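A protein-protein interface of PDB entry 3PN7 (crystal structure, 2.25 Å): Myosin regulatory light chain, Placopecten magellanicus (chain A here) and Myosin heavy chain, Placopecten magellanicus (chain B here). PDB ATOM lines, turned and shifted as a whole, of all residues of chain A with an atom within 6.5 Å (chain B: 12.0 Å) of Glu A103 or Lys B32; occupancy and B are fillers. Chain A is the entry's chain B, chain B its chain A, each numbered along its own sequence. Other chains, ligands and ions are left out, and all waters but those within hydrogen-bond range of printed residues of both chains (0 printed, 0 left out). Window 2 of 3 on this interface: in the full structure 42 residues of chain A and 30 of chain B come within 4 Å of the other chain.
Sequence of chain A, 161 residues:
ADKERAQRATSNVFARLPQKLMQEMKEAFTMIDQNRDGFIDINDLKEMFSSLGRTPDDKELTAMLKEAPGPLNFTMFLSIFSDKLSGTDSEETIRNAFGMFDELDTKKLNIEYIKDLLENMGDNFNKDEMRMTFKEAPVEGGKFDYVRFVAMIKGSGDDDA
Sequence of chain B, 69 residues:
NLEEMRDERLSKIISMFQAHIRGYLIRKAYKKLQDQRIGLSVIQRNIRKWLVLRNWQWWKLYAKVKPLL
The backbone carbonyl oxygen (O) of Met A100 lies within hydrogen-bond range of the side-chain amide nitrogen (NE2) of Gln B36 (3.1 Å).
The side-chain amino group of Lys B31 lies within salt-bridge range of the side-chain carboxylate of Asp B35, 3.2 Å away.
Printed residues of chain B within 4 Å of Met A100: Asp B35 (3.5 Å), Gln B36 (3.1 Å) and Gly B39 (3.9 Å). Asp A102 touches none of the printed residues of chain B. Glu A103 touches one residue of chain B. No residue of chain B comes within 4 Å of Leu A104. No residue of chain B comes within 4 Å of Asp A105. Lys B28 touches none of the printed residues of chain A. Of the printed residues of chain A, Asp B35 touches Met A100. Printed residues of chain A within 4 Å of Gln B36: Met A100 (3.1 Å) and Phe A101 (3.2 Å). Of the printed residues of chain A, Gly B39 touches Met A100 (3.9 Å). Of the printed residues of chain A, Leu B40 touches Phe A101. Printed residues of chain A within 4 Å of Ile B43: Phe A98.
Of the 20 printed residues of chain B, 6 touch a printed residue of chain A. Among the printed residues, no Asp or Glu carboxylate lies within 4 Å of a Lys or Arg side-chain nitrogen of the other chain.
Among the printed residues, pairs that only touch across the chains: Phe A98 with Ile B43, Met A100 with Asp B35, Met A100 with Gly B39, Phe A101 with Gln B36, Phe A101 with Leu B40 and Glu A103 with Lys B32.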
ATOM      1  N   PHE A  98     -13.422 -14.745   0.362  1.00  0.00           N
ATOM      2  CA  PHE A  98     -12.425 -15.685   0.842  1.00  0.00           C
ATOM      3  C   PHE A  98     -11.024 -15.403   0.238  1.00  0.00           C
ATOM      4  O   PHE A  98     -10.004 -15.518   0.928  1.00  0.00           O
ATOM      5  CB  PHE A  98     -12.856 -17.131   0.550  1.00  0.00           C
ATOM      6  CG  PHE A  98     -13.810 -17.721   1.577  1.00  0.00           C
ATOM      7  CD1 PHE A  98     -13.363 -18.075   2.846  1.00  0.00           C
ATOM      8  CD2 PHE A  98     -15.146 -17.963   1.254  1.00  0.00           C
ATOM      9  CE1 PHE A  98     -14.232 -18.645   3.784  1.00  0.00           C
ATOM     10  CE2 PHE A  98     -16.026 -18.523   2.184  1.00  0.00           C
ATOM     11  CZ  PHE A  98     -15.573 -18.868   3.445  1.00  0.00           C
ATOM     12  N   GLY A  99     -10.978 -15.029  -1.042  1.00  0.00           N
ATOM     13  CA  GLY A  99      -9.713 -14.790  -1.735  1.00  0.00           C
ATOM     14  C   GLY A  99      -8.903 -13.707  -1.033  1.00  0.00           C
ATOM     15  O   GLY A  99      -7.681 -13.718  -1.004  1.00  0.00           O
ATOM     16  N   MET A 100      -9.624 -12.764  -0.451  1.00  0.00           N
ATOM     17  CA  MET A 100      -9.049 -11.668   0.301  1.00  0.00           C
ATOM     18  C   MET A 100      -8.035 -12.119   1.350  1.00  0.00           C
ATOM     19  O   MET A 100      -7.160 -11.344   1.744  1.00  0.00           O
ATOM     20  CB  MET A 100     -10.183 -10.955   1.028  1.00  0.00           C
ATOM     21  CG  MET A 100     -10.051  -9.482   1.043  1.00  0.00           C
ATOM     22  SD  MET A 100     -10.531  -8.904  -0.568  1.00  0.00           S
ATOM     23  CE  MET A 100     -12.311  -8.901  -0.324  1.00  0.00           C
ATOM     24  N   PHE A 101      -8.189 -13.354   1.826  1.00  0.00           N
ATOM     25  CA  PHE A 101      -7.362 -13.873   2.906  1.00  0.00           C
ATOM     26  C   PHE A 101      -6.457 -14.978   2.373  1.00  0.00           C
ATOM     27  O   PHE A 101      -5.794 -15.685   3.140  1.00  0.00           O
ATOM     28  CB  PHE A 101      -8.238 -14.398   4.056  1.00  0.00           C
ATOM     29  CG  PHE A 101      -9.202 -13.374   4.600  1.00  0.00           C
ATOM     30  CD1 PHE A 101     -10.506 -13.319   4.139  1.00  0.00           C
ATOM     31  CD2 PHE A 101      -8.799 -12.459   5.561  1.00  0.00           C
ATOM     32  CE1 PHE A 101     -11.397 -12.372   4.639  1.00  0.00           C
ATOM     33  CE2 PHE A 101      -9.677 -11.519   6.071  1.00  0.00           C
ATOM     34  CZ  PHE A 101     -10.977 -11.461   5.599  1.00  0.00           C
ATOM     35  N   ASP A 102      -6.446 -15.113   1.049  1.00  0.00           N
ATOM     36  CA  ASP A 102      -5.666 -16.140   0.350  1.00  0.00           C
ATOM     37  C   ASP A 102      -4.752 -15.422  -0.659  1.00  0.00           C
ATOM     38  O   ASP A 102      -4.984 -15.446  -1.866  1.00  0.00           O
ATOM     39  CB  ASP A 102      -6.615 -17.134  -0.345  1.00  0.00           C
ATOM     40  CG  ASP A 102      -5.880 -18.171  -1.222  1.00  0.00           C
ATOM     41  OD1 ASP A 102      -4.649 -18.319  -1.086  1.00  0.00           O
ATOM     42  OD2 ASP A 102      -6.548 -18.854  -2.037  1.00  0.00           O
ATOM     43  N   GLU A 103      -3.733 -14.753  -0.132  1.00  0.00           N
ATOM     44  CA  GLU A 103      -2.882 -13.867  -0.915  1.00  0.00           C
ATOM     45  C   GLU A 103      -2.328 -14.566  -2.153  1.00  0.00           C
ATOM     46  O   GLU A 103      -2.414 -14.044  -3.267  1.00  0.00           O
ATOM     47  CB  GLU A 103      -1.733 -13.373  -0.038  1.00  0.00           C
ATOM     48  CG  GLU A 103      -1.786 -11.890   0.301  1.00  0.00           C
ATOM     49  CD  GLU A 103      -1.118 -11.034  -0.765  1.00  0.00           C
ATOM     50  OE1 GLU A 103       0.138 -10.977  -0.790  1.00  0.00           O
ATOM     51  OE2 GLU A 103      -1.847 -10.427  -1.584  1.00  0.00           O
ATOM     52  N   LEU A 104      -1.769 -15.756  -1.939  1.00  0.00           N
ATOM     53  CA  LEU A 104      -1.134 -16.532  -2.994  1.00  0.00           C
ATOM     54  C   LEU A 104      -2.107 -17.351  -3.844  1.00  0.00           C
ATOM     55  O   LEU A 104      -1.675 -18.177  -4.651  1.00  0.00           O
ATOM     56  CB  LEU A 104      -0.078 -17.460  -2.393  1.00  0.00           C
ATOM     57  CG  LEU A 104       0.931 -16.766  -1.476  1.00  0.00           C
ATOM     58  CD1 LEU A 104       1.684 -17.780  -0.628  1.00  0.00           C
ATOM     59  CD2 LEU A 104       1.895 -15.899  -2.271  1.00  0.00           C
ATOM     60  N   ASP A 105      -3.410 -17.145  -3.651  1.00  0.00           N
ATOM     61  CA  ASP A 105      -4.429 -17.783  -4.491  1.00  0.00           C
ATOM     62  C   ASP A 105      -4.309 -19.312  -4.526  1.00  0.00           C
ATOM     63  O   ASP A 105      -4.388 -19.921  -5.589  1.00  0.00           O
ATOM     64  CB  ASP A 105      -4.355 -17.227  -5.920  1.00  0.00           C
ATOM     65  CG  ASP A 105      -5.694 -17.272  -6.640  1.00  0.00           C
ATOM     66  OD1 ASP A 105      -6.742 -17.457  -5.975  1.00  0.00           O
ATOM     67  OD2 ASP A 105      -5.698 -17.111  -7.878  1.00  0.00           O
ATOM     68  N   THR A 106      -4.119 -19.926  -3.362  1.00  0.00           N
ATOM     69  CA  THR A 106      -4.079 -21.380  -3.265  1.00  0.00           C
ATOM     70  C   THR A 106      -5.465 -21.993  -3.342  1.00  0.00           C
ATOM     71  O   THR A 106      -5.595 -23.204  -3.547  1.00  0.00           O
ATOM     72  CB  THR A 106      -3.460 -21.832  -1.932  1.00  0.00           C
ATOM     73  OG1 THR A 106      -4.267 -21.356  -0.842  1.00  0.00           O
ATOM     74  CG2 THR A 106      -2.058 -21.280  -1.806  1.00  0.00           C
ATOM     75  N   LEU A 109      -7.561 -22.147   2.737  1.00  0.00           N
ATOM     76  CA  LEU A 109      -7.230 -21.309   3.874  1.00  0.00           C
ATOM     77  C   LEU A 109      -6.810 -22.285   4.975  1.00  0.00           C
ATOM     78  O   LEU A 109      -7.411 -23.350   5.113  1.00  0.00           O
ATOM     79  CB  LEU A 109      -8.489 -20.545   4.306  1.00  0.00           C
ATOM     80  CG  LEU A 109      -8.573 -19.028   4.247  1.00  0.00           C
ATOM     81  CD1 LEU A 109      -7.703 -18.468   3.127  1.00  0.00           C
ATOM     82  CD2 LEU A 109     -10.027 -18.533   4.130  1.00  0.00           C
ATOM     83  N   TYR B  24       4.881   3.453   8.325  1.00  0.00           N
ATOM     84  CA  TYR B  24       4.855   2.989   6.938  1.00  0.00           C
ATOM     85  C   TYR B  24       4.163   1.628   6.827  1.00  0.00           C
ATOM     86  O   TYR B  24       3.248   1.451   6.035  1.00  0.00           O
ATOM     87  CB  TYR B  24       6.292   2.880   6.417  1.00  0.00           C
ATOM     88  CG  TYR B  24       6.467   2.597   4.938  1.00  0.00           C
ATOM     89  CD1 TYR B  24       6.077   1.388   4.376  1.00  0.00           C
ATOM     90  CD2 TYR B  24       7.084   3.533   4.106  1.00  0.00           C
ATOM     91  CE1 TYR B  24       6.269   1.132   3.014  1.00  0.00           C
ATOM     92  CE2 TYR B  24       7.278   3.288   2.754  1.00  0.00           C
ATOM     93  CZ  TYR B  24       6.869   2.085   2.215  1.00  0.00           C
ATOM     94  OH  TYR B  24       7.062   1.856   0.869  1.00  0.00           O
ATOM     95  N   LEU B  25       4.614   0.671   7.630  1.00  0.00           N
ATOM     96  CA  LEU B  25       4.100  -0.691   7.573  1.00  0.00           C
ATOM     97  C   LEU B  25       2.585  -0.740   7.747  1.00  0.00           C
ATOM     98  O   LEU B  25       1.895  -1.394   6.977  1.00  0.00           O
ATOM     99  CB  LEU B  25       4.785  -1.571   8.625  1.00  0.00           C
ATOM    100  CG  LEU B  25       5.978  -2.419   8.177  1.00  0.00           C
ATOM    101  CD1 LEU B  25       6.527  -1.990   6.846  1.00  0.00           C
ATOM    102  CD2 LEU B  25       7.066  -2.459   9.209  1.00  0.00           C
ATOM    103  N   ILE B  26       2.077  -0.044   8.765  1.00  0.00           N
ATOM    104  CA  ILE B  26       0.647  -0.034   9.026  1.00  0.00           C
ATOM    105  C   ILE B  26      -0.129   0.666   7.912  1.00  0.00           C
ATOM    106  O   ILE B  26      -1.146   0.168   7.461  1.00  0.00           O
ATOM    107  CB  ILE B  26       0.298   0.563  10.401  1.00  0.00           C
ATOM    108  CG1 ILE B  26       0.948  -0.269  11.504  1.00  0.00           C
ATOM    109  CG2 ILE B  26      -1.203   0.507  10.637  1.00  0.00           C
ATOM    110  CD1 ILE B  26       0.650  -1.759  11.376  1.00  0.00           C
ATOM    111  N   ARG B  27       0.348   1.822   7.475  1.00  0.00           N
ATOM    112  CA  ARG B  27      -0.357   2.568   6.440  1.00  0.00           C
ATOM    113  C   ARG B  27      -0.408   1.802   5.120  1.00  0.00           C
ATOM    114  O   ARG B  27      -1.360   1.931   4.358  1.00  0.00           O
ATOM    115  CB  ARG B  27       0.256   3.956   6.252  1.00  0.00           C
ATOM    116  CG  ARG B  27      -0.221   4.964   7.283  1.00  0.00           C
ATOM    117  CD  ARG B  27       0.361   6.341   7.044  1.00  0.00           C
ATOM    118  NE  ARG B  27       1.802   6.370   7.261  1.00  0.00           N
ATOM    119  CZ  ARG B  27       2.381   6.626   8.428  1.00  0.00           C
ATOM    120  NH1 ARG B  27       1.645   6.874   9.499  1.00  0.00           N
ATOM    121  NH2 ARG B  27       3.702   6.632   8.525  1.00  0.00           N
ATOM    122  N   LYS B  28       0.615   0.997   4.864  1.00  0.00           N
ATOM    123  CA  LYS B  28       0.670   0.196   3.651  1.00  0.00           C
ATOM    124  C   LYS B  28      -0.357  -0.933   3.685  1.00  0.00           C
ATOM    125  O   LYS B  28      -0.870  -1.350   2.652  1.00  0.00           O
ATOM    126  CB  LYS B  28       2.074  -0.380   3.461  1.00  0.00           C
ATOM    127  CG  LYS B  28       2.176  -1.413   2.361  1.00  0.00           C
ATOM    128  CD  LYS B  28       2.177  -0.755   0.995  1.00  0.00           C
ATOM    129  CE  LYS B  28       2.032  -1.782  -0.113  1.00  0.00           C
ATOM    130  NZ  LYS B  28       0.621  -2.207  -0.290  1.00  0.00           N
ATOM    131  N   ALA B  29      -0.647  -1.419   4.886  1.00  0.00           N
ATOM    132  CA  ALA B  29      -1.590  -2.518   5.085  1.00  0.00           C
ATOM    133  C   ALA B  29      -3.046  -2.053   5.193  1.00  0.00           C
ATOM    134  O   ALA B  29      -3.965  -2.873   5.200  1.00  0.00           O
ATOM    135  CB  ALA B  29      -1.194  -3.337   6.332  1.00  0.00           C
ATOM    136  N   TYR B  30      -3.250  -0.738   5.255  1.00  0.00           N
ATOM    137  CA  TYR B  30      -4.577  -0.177   5.527  1.00  0.00           C
ATOM    138  C   TYR B  30      -5.687  -0.529   4.521  1.00  0.00           C
ATOM    139  O   TYR B  30      -6.804  -0.883   4.913  1.00  0.00           O
ATOM    140  CB  TYR B  30      -4.492   1.336   5.670  1.00  0.00           C
ATOM    141  CG  TYR B  30      -5.803   1.950   6.073  1.00  0.00           C
ATOM    142  CD1 TYR B  30      -6.304   1.769   7.358  1.00  0.00           C
ATOM    143  CD2 TYR B  30      -6.554   2.696   5.170  1.00  0.00           C
ATOM    144  CE1 TYR B  30      -7.499   2.330   7.746  1.00  0.00           C
ATOM    145  CE2 TYR B  30      -7.771   3.261   5.554  1.00  0.00           C
ATOM    146  CZ  TYR B  30      -8.232   3.072   6.850  1.00  0.00           C
ATOM    147  OH  TYR B  30      -9.429   3.615   7.260  1.00  0.00           O
ATOM    148  N   LYS B  31      -5.383  -0.402   3.234  1.00  0.00           N
ATOM    149  CA  LYS B  31      -6.328  -0.706   2.160  1.00  0.00           C
ATOM    150  C   LYS B  31      -6.778  -2.185   2.170  1.00  0.00           C
ATOM    151  O   LYS B  31      -7.963  -2.500   2.021  1.00  0.00           O
ATOM    152  CB  LYS B  31      -5.694  -0.346   0.814  1.00  0.00           C
ATOM    153  CG  LYS B  31      -6.459  -0.869  -0.407  1.00  0.00           C
ATOM    154  CD  LYS B  31      -7.827  -0.188  -0.547  1.00  0.00           C
ATOM    155  CE  LYS B  31      -8.650  -0.827  -1.677  1.00  0.00           C
ATOM    156  NZ  LYS B  31     -10.033  -0.254  -1.769  1.00  0.00           N
ATOM    157  N   LYS B  32      -5.826  -3.088   2.352  1.00  0.00           N
ATOM    158  CA  LYS B  32      -6.132  -4.503   2.441  1.00  0.00           C
ATOM    159  C   LYS B  32      -7.028  -4.767   3.657  1.00  0.00           C
ATOM    160  O   LYS B  32      -7.918  -5.623   3.628  1.00  0.00           O
ATOM    161  CB  LYS B  32      -4.830  -5.298   2.552  1.00  0.00           C
ATOM    162  CG  LYS B  32      -4.983  -6.817   2.503  1.00  0.00           C
ATOM    163  CD  LYS B  32      -3.646  -7.510   2.844  1.00  0.00           C
ATOM    164  CE  LYS B  32      -3.618  -8.996   2.428  1.00  0.00           C
ATOM    165  NZ  LYS B  32      -2.349  -9.704   2.838  1.00  0.00           N
ATOM    166  N   LEU B  33      -6.782  -4.024   4.728  1.00  0.00           N
ATOM    167  CA  LEU B  33      -7.552  -4.175   5.955  1.00  0.00           C
ATOM    168  C   LEU B  33      -9.007  -3.779   5.736  1.00  0.00           C
ATOM    169  O   LEU B  33      -9.915  -4.456   6.214  1.00  0.00           O
ATOM    170  CB  LEU B  33      -6.958  -3.299   7.047  1.00  0.00           C
ATOM    171  CG  LEU B  33      -7.057  -3.818   8.468  1.00  0.00           C
ATOM    172  CD1 LEU B  33      -6.611  -5.289   8.534  1.00  0.00           C
ATOM    173  CD2 LEU B  33      -6.201  -2.921   9.388  1.00  0.00           C
ATOM    174  N   GLN B  34      -9.222  -2.672   5.029  1.00  0.00           N
ATOM    175  CA  GLN B  34     -10.562  -2.256   4.654  1.00  0.00           C
ATOM    176  C   GLN B  34     -11.210  -3.279   3.736  1.00  0.00           C
ATOM    177  O   GLN B  34     -12.382  -3.614   3.899  1.00  0.00           O
ATOM    178  CB  GLN B  34     -10.527  -0.907   3.944  1.00  0.00           C
ATOM    179  CG  GLN B  34      -9.940   0.206   4.798  1.00  0.00           C
ATOM    180  CD  GLN B  34     -10.364   1.590   4.313  1.00  0.00           C
ATOM    181  OE1 GLN B  34     -10.910   2.395   5.088  1.00  0.00           O
ATOM    182  NE2 GLN B  34     -10.127   1.872   3.025  1.00  0.00           N
ATOM    183  N   ASP B  35     -10.452  -3.762   2.758  1.00  0.00           N
ATOM    184  CA  ASP B  35     -10.983  -4.756   1.838  1.00  0.00           C
ATOM    185  C   ASP B  35     -11.340  -6.023   2.595  1.00  0.00           C
ATOM    186  O   ASP B  35     -12.353  -6.640   2.327  1.00  0.00           O
ATOM    187  CB  ASP B  35      -9.966  -5.108   0.760  1.00  0.00           C
ATOM    188  CG  ASP B  35      -9.827  -4.033  -0.295  1.00  0.00           C
ATOM    189  OD1 ASP B  35     -10.638  -3.089  -0.322  1.00  0.00           O
ATOM    190  OD2 ASP B  35      -8.884  -4.143  -1.107  1.00  0.00           O
ATOM    191  N   GLN B  36     -10.494  -6.416   3.539  1.00  0.00           N
ATOM    192  CA  GLN B  36     -10.696  -7.683   4.226  1.00  0.00           C
ATOM    193  C   GLN B  36     -11.874  -7.615   5.182  1.00  0.00           C
ATOM    194  O   GLN B  36     -12.504  -8.629   5.464  1.00  0.00           O
ATOM    195  CB  GLN B  36      -9.442  -8.107   4.973  1.00  0.00           C
ATOM    196  CG  GLN B  36      -8.418  -8.824   4.106  1.00  0.00           C
ATOM    197  CD  GLN B  36      -7.105  -9.012   4.837  1.00  0.00           C
ATOM    198  OE1 GLN B  36      -6.880  -8.403   5.875  1.00  0.00           O
ATOM    199  NE2 GLN B  36      -6.242  -9.854   4.306  1.00  0.00           N
ATOM    200  N   ARG B  37     -12.153  -6.417   5.683  1.00  0.00           N
ATOM    201  CA  ARG B  37     -13.317  -6.192   6.509  1.00  0.00           C
ATOM    202  C   ARG B  37     -14.607  -6.499   5.731  1.00  0.00           C
ATOM    203  O   ARG B  37     -15.482  -7.204   6.229  1.00  0.00           O
ATOM    204  CB  ARG B  37     -13.339  -4.751   6.993  1.00  0.00           C
ATOM    205  CG  ARG B  37     -14.631  -4.357   7.679  1.00  0.00           C
ATOM    206  CD  ARG B  37     -14.821  -2.863   7.518  1.00  0.00           C
ATOM    207  NE  ARG B  37     -15.401  -2.218   8.690  1.00  0.00           N
ATOM    208  CZ  ARG B  37     -15.421  -0.899   8.869  1.00  0.00           C
ATOM    209  NH1 ARG B  37     -14.886  -0.103   7.949  1.00  0.00           N
ATOM    210  NH2 ARG B  37     -15.964  -0.380   9.968  1.00  0.00           N
ATOM    211  N   ILE B  38     -14.720  -5.952   4.522  1.00  0.00           N
ATOM    212  CA  ILE B  38     -15.827  -6.273   3.614  1.00  0.00           C
ATOM    213  C   ILE B  38     -15.869  -7.769   3.315  1.00  0.00           C
ATOM    214  O   ILE B  38     -16.924  -8.394   3.390  1.00  0.00           O
ATOM    215  CB  ILE B  38     -15.700  -5.508   2.267  1.00  0.00           C
ATOM    216  CG1 ILE B  38     -16.044  -4.037   2.458  1.00  0.00           C
ATOM    217  CG2 ILE B  38     -16.583  -6.131   1.178  1.00  0.00           C
ATOM    218  CD1 ILE B  38     -15.464  -3.153   1.381  1.00  0.00           C
ATOM    219  N   GLY B  39     -14.725  -8.345   2.967  1.00  0.00           N
ATOM    220  CA  GLY B  39     -14.672  -9.773   2.712  1.00  0.00           C
ATOM    221  C   GLY B  39     -15.210 -10.618   3.873  1.00  0.00           C
ATOM    222  O   GLY B  39     -15.994 -11.547   3.655  1.00  0.00           O
ATOM    223  N   LEU B  40     -14.777 -10.328   5.100  1.00  0.00           N
ATOM    224  CA  LEU B  40     -15.218 -11.110   6.260  1.00  0.00           C
ATOM    225  C   LEU B  40     -16.704 -10.864   6.583  1.00  0.00           C
ATOM    226  O   LEU B  40     -17.412 -11.789   6.974  1.00  0.00           O
ATOM    227  CB  LEU B  40     -14.353 -10.820   7.490  1.00  0.00           C
ATOM    228  CG  LEU B  40     -14.760 -11.536   8.780  1.00  0.00           C
ATOM    229  CD1 LEU B  40     -14.612 -13.035   8.639  1.00  0.00           C
ATOM    230  CD2 LEU B  40     -13.922 -11.024   9.974  1.00  0.00           C
ATOM    231  N   SER B  41     -17.164  -9.621   6.442  1.00  0.00           N
ATOM    232  CA  SER B  41     -18.588  -9.333   6.542  1.00  0.00           C
ATOM    233  C   SER B  41     -19.383 -10.200   5.566  1.00  0.00           C
ATOM    234  O   SER B  41     -20.376 -10.817   5.945  1.00  0.00           O
ATOM    235  CB  SER B  41     -18.869  -7.864   6.237  1.00  0.00           C
ATOM    236  OG  SER B  41     -18.191  -7.032   7.149  1.00  0.00           O
ATOM    237  N   VAL B  42     -18.947 -10.240   4.312  1.00  0.00           N
ATOM    238  CA  VAL B  42     -19.593 -11.089   3.310  1.00  0.00           C
ATOM    239  C   VAL B  42     -19.621 -12.542   3.742  1.00  0.00           C
ATOM    240  O   VAL B  42     -20.650 -13.221   3.627  1.00  0.00           O
ATOM    241  CB  VAL B  42     -18.864 -11.055   1.969  1.00  0.00           C
ATOM    242  CG1 VAL B  42     -19.361 -12.185   1.082  1.00  0.00           C
ATOM    243  CG2 VAL B  42     -19.017  -9.696   1.290  1.00  0.00           C
ATOM    244  N   ILE B  43     -18.486 -13.032   4.226  1.00  0.00           N
ATOM    245  CA  ILE B  43     -18.395 -14.429   4.651  1.00  0.00           C
ATOM    246  C   ILE B  43     -19.284 -14.772   5.858  1.00  0.00           C
ATOM    247  O   ILE B  43     -19.967 -15.791   5.857  1.00  0.00           O
ATOM    248  CB  ILE B  43     -16.948 -14.810   4.981  1.00  0.00           C
ATOM    249  CG1 ILE B  43     -16.100 -14.858   3.711  1.00  0.00           C
ATOM    250  CG2 ILE B  43     -16.898 -16.144   5.684  1.00  0.00           C
ATOM    251  CD1 ILE B  43     -14.591 -14.783   3.999  1.00  0.00           C
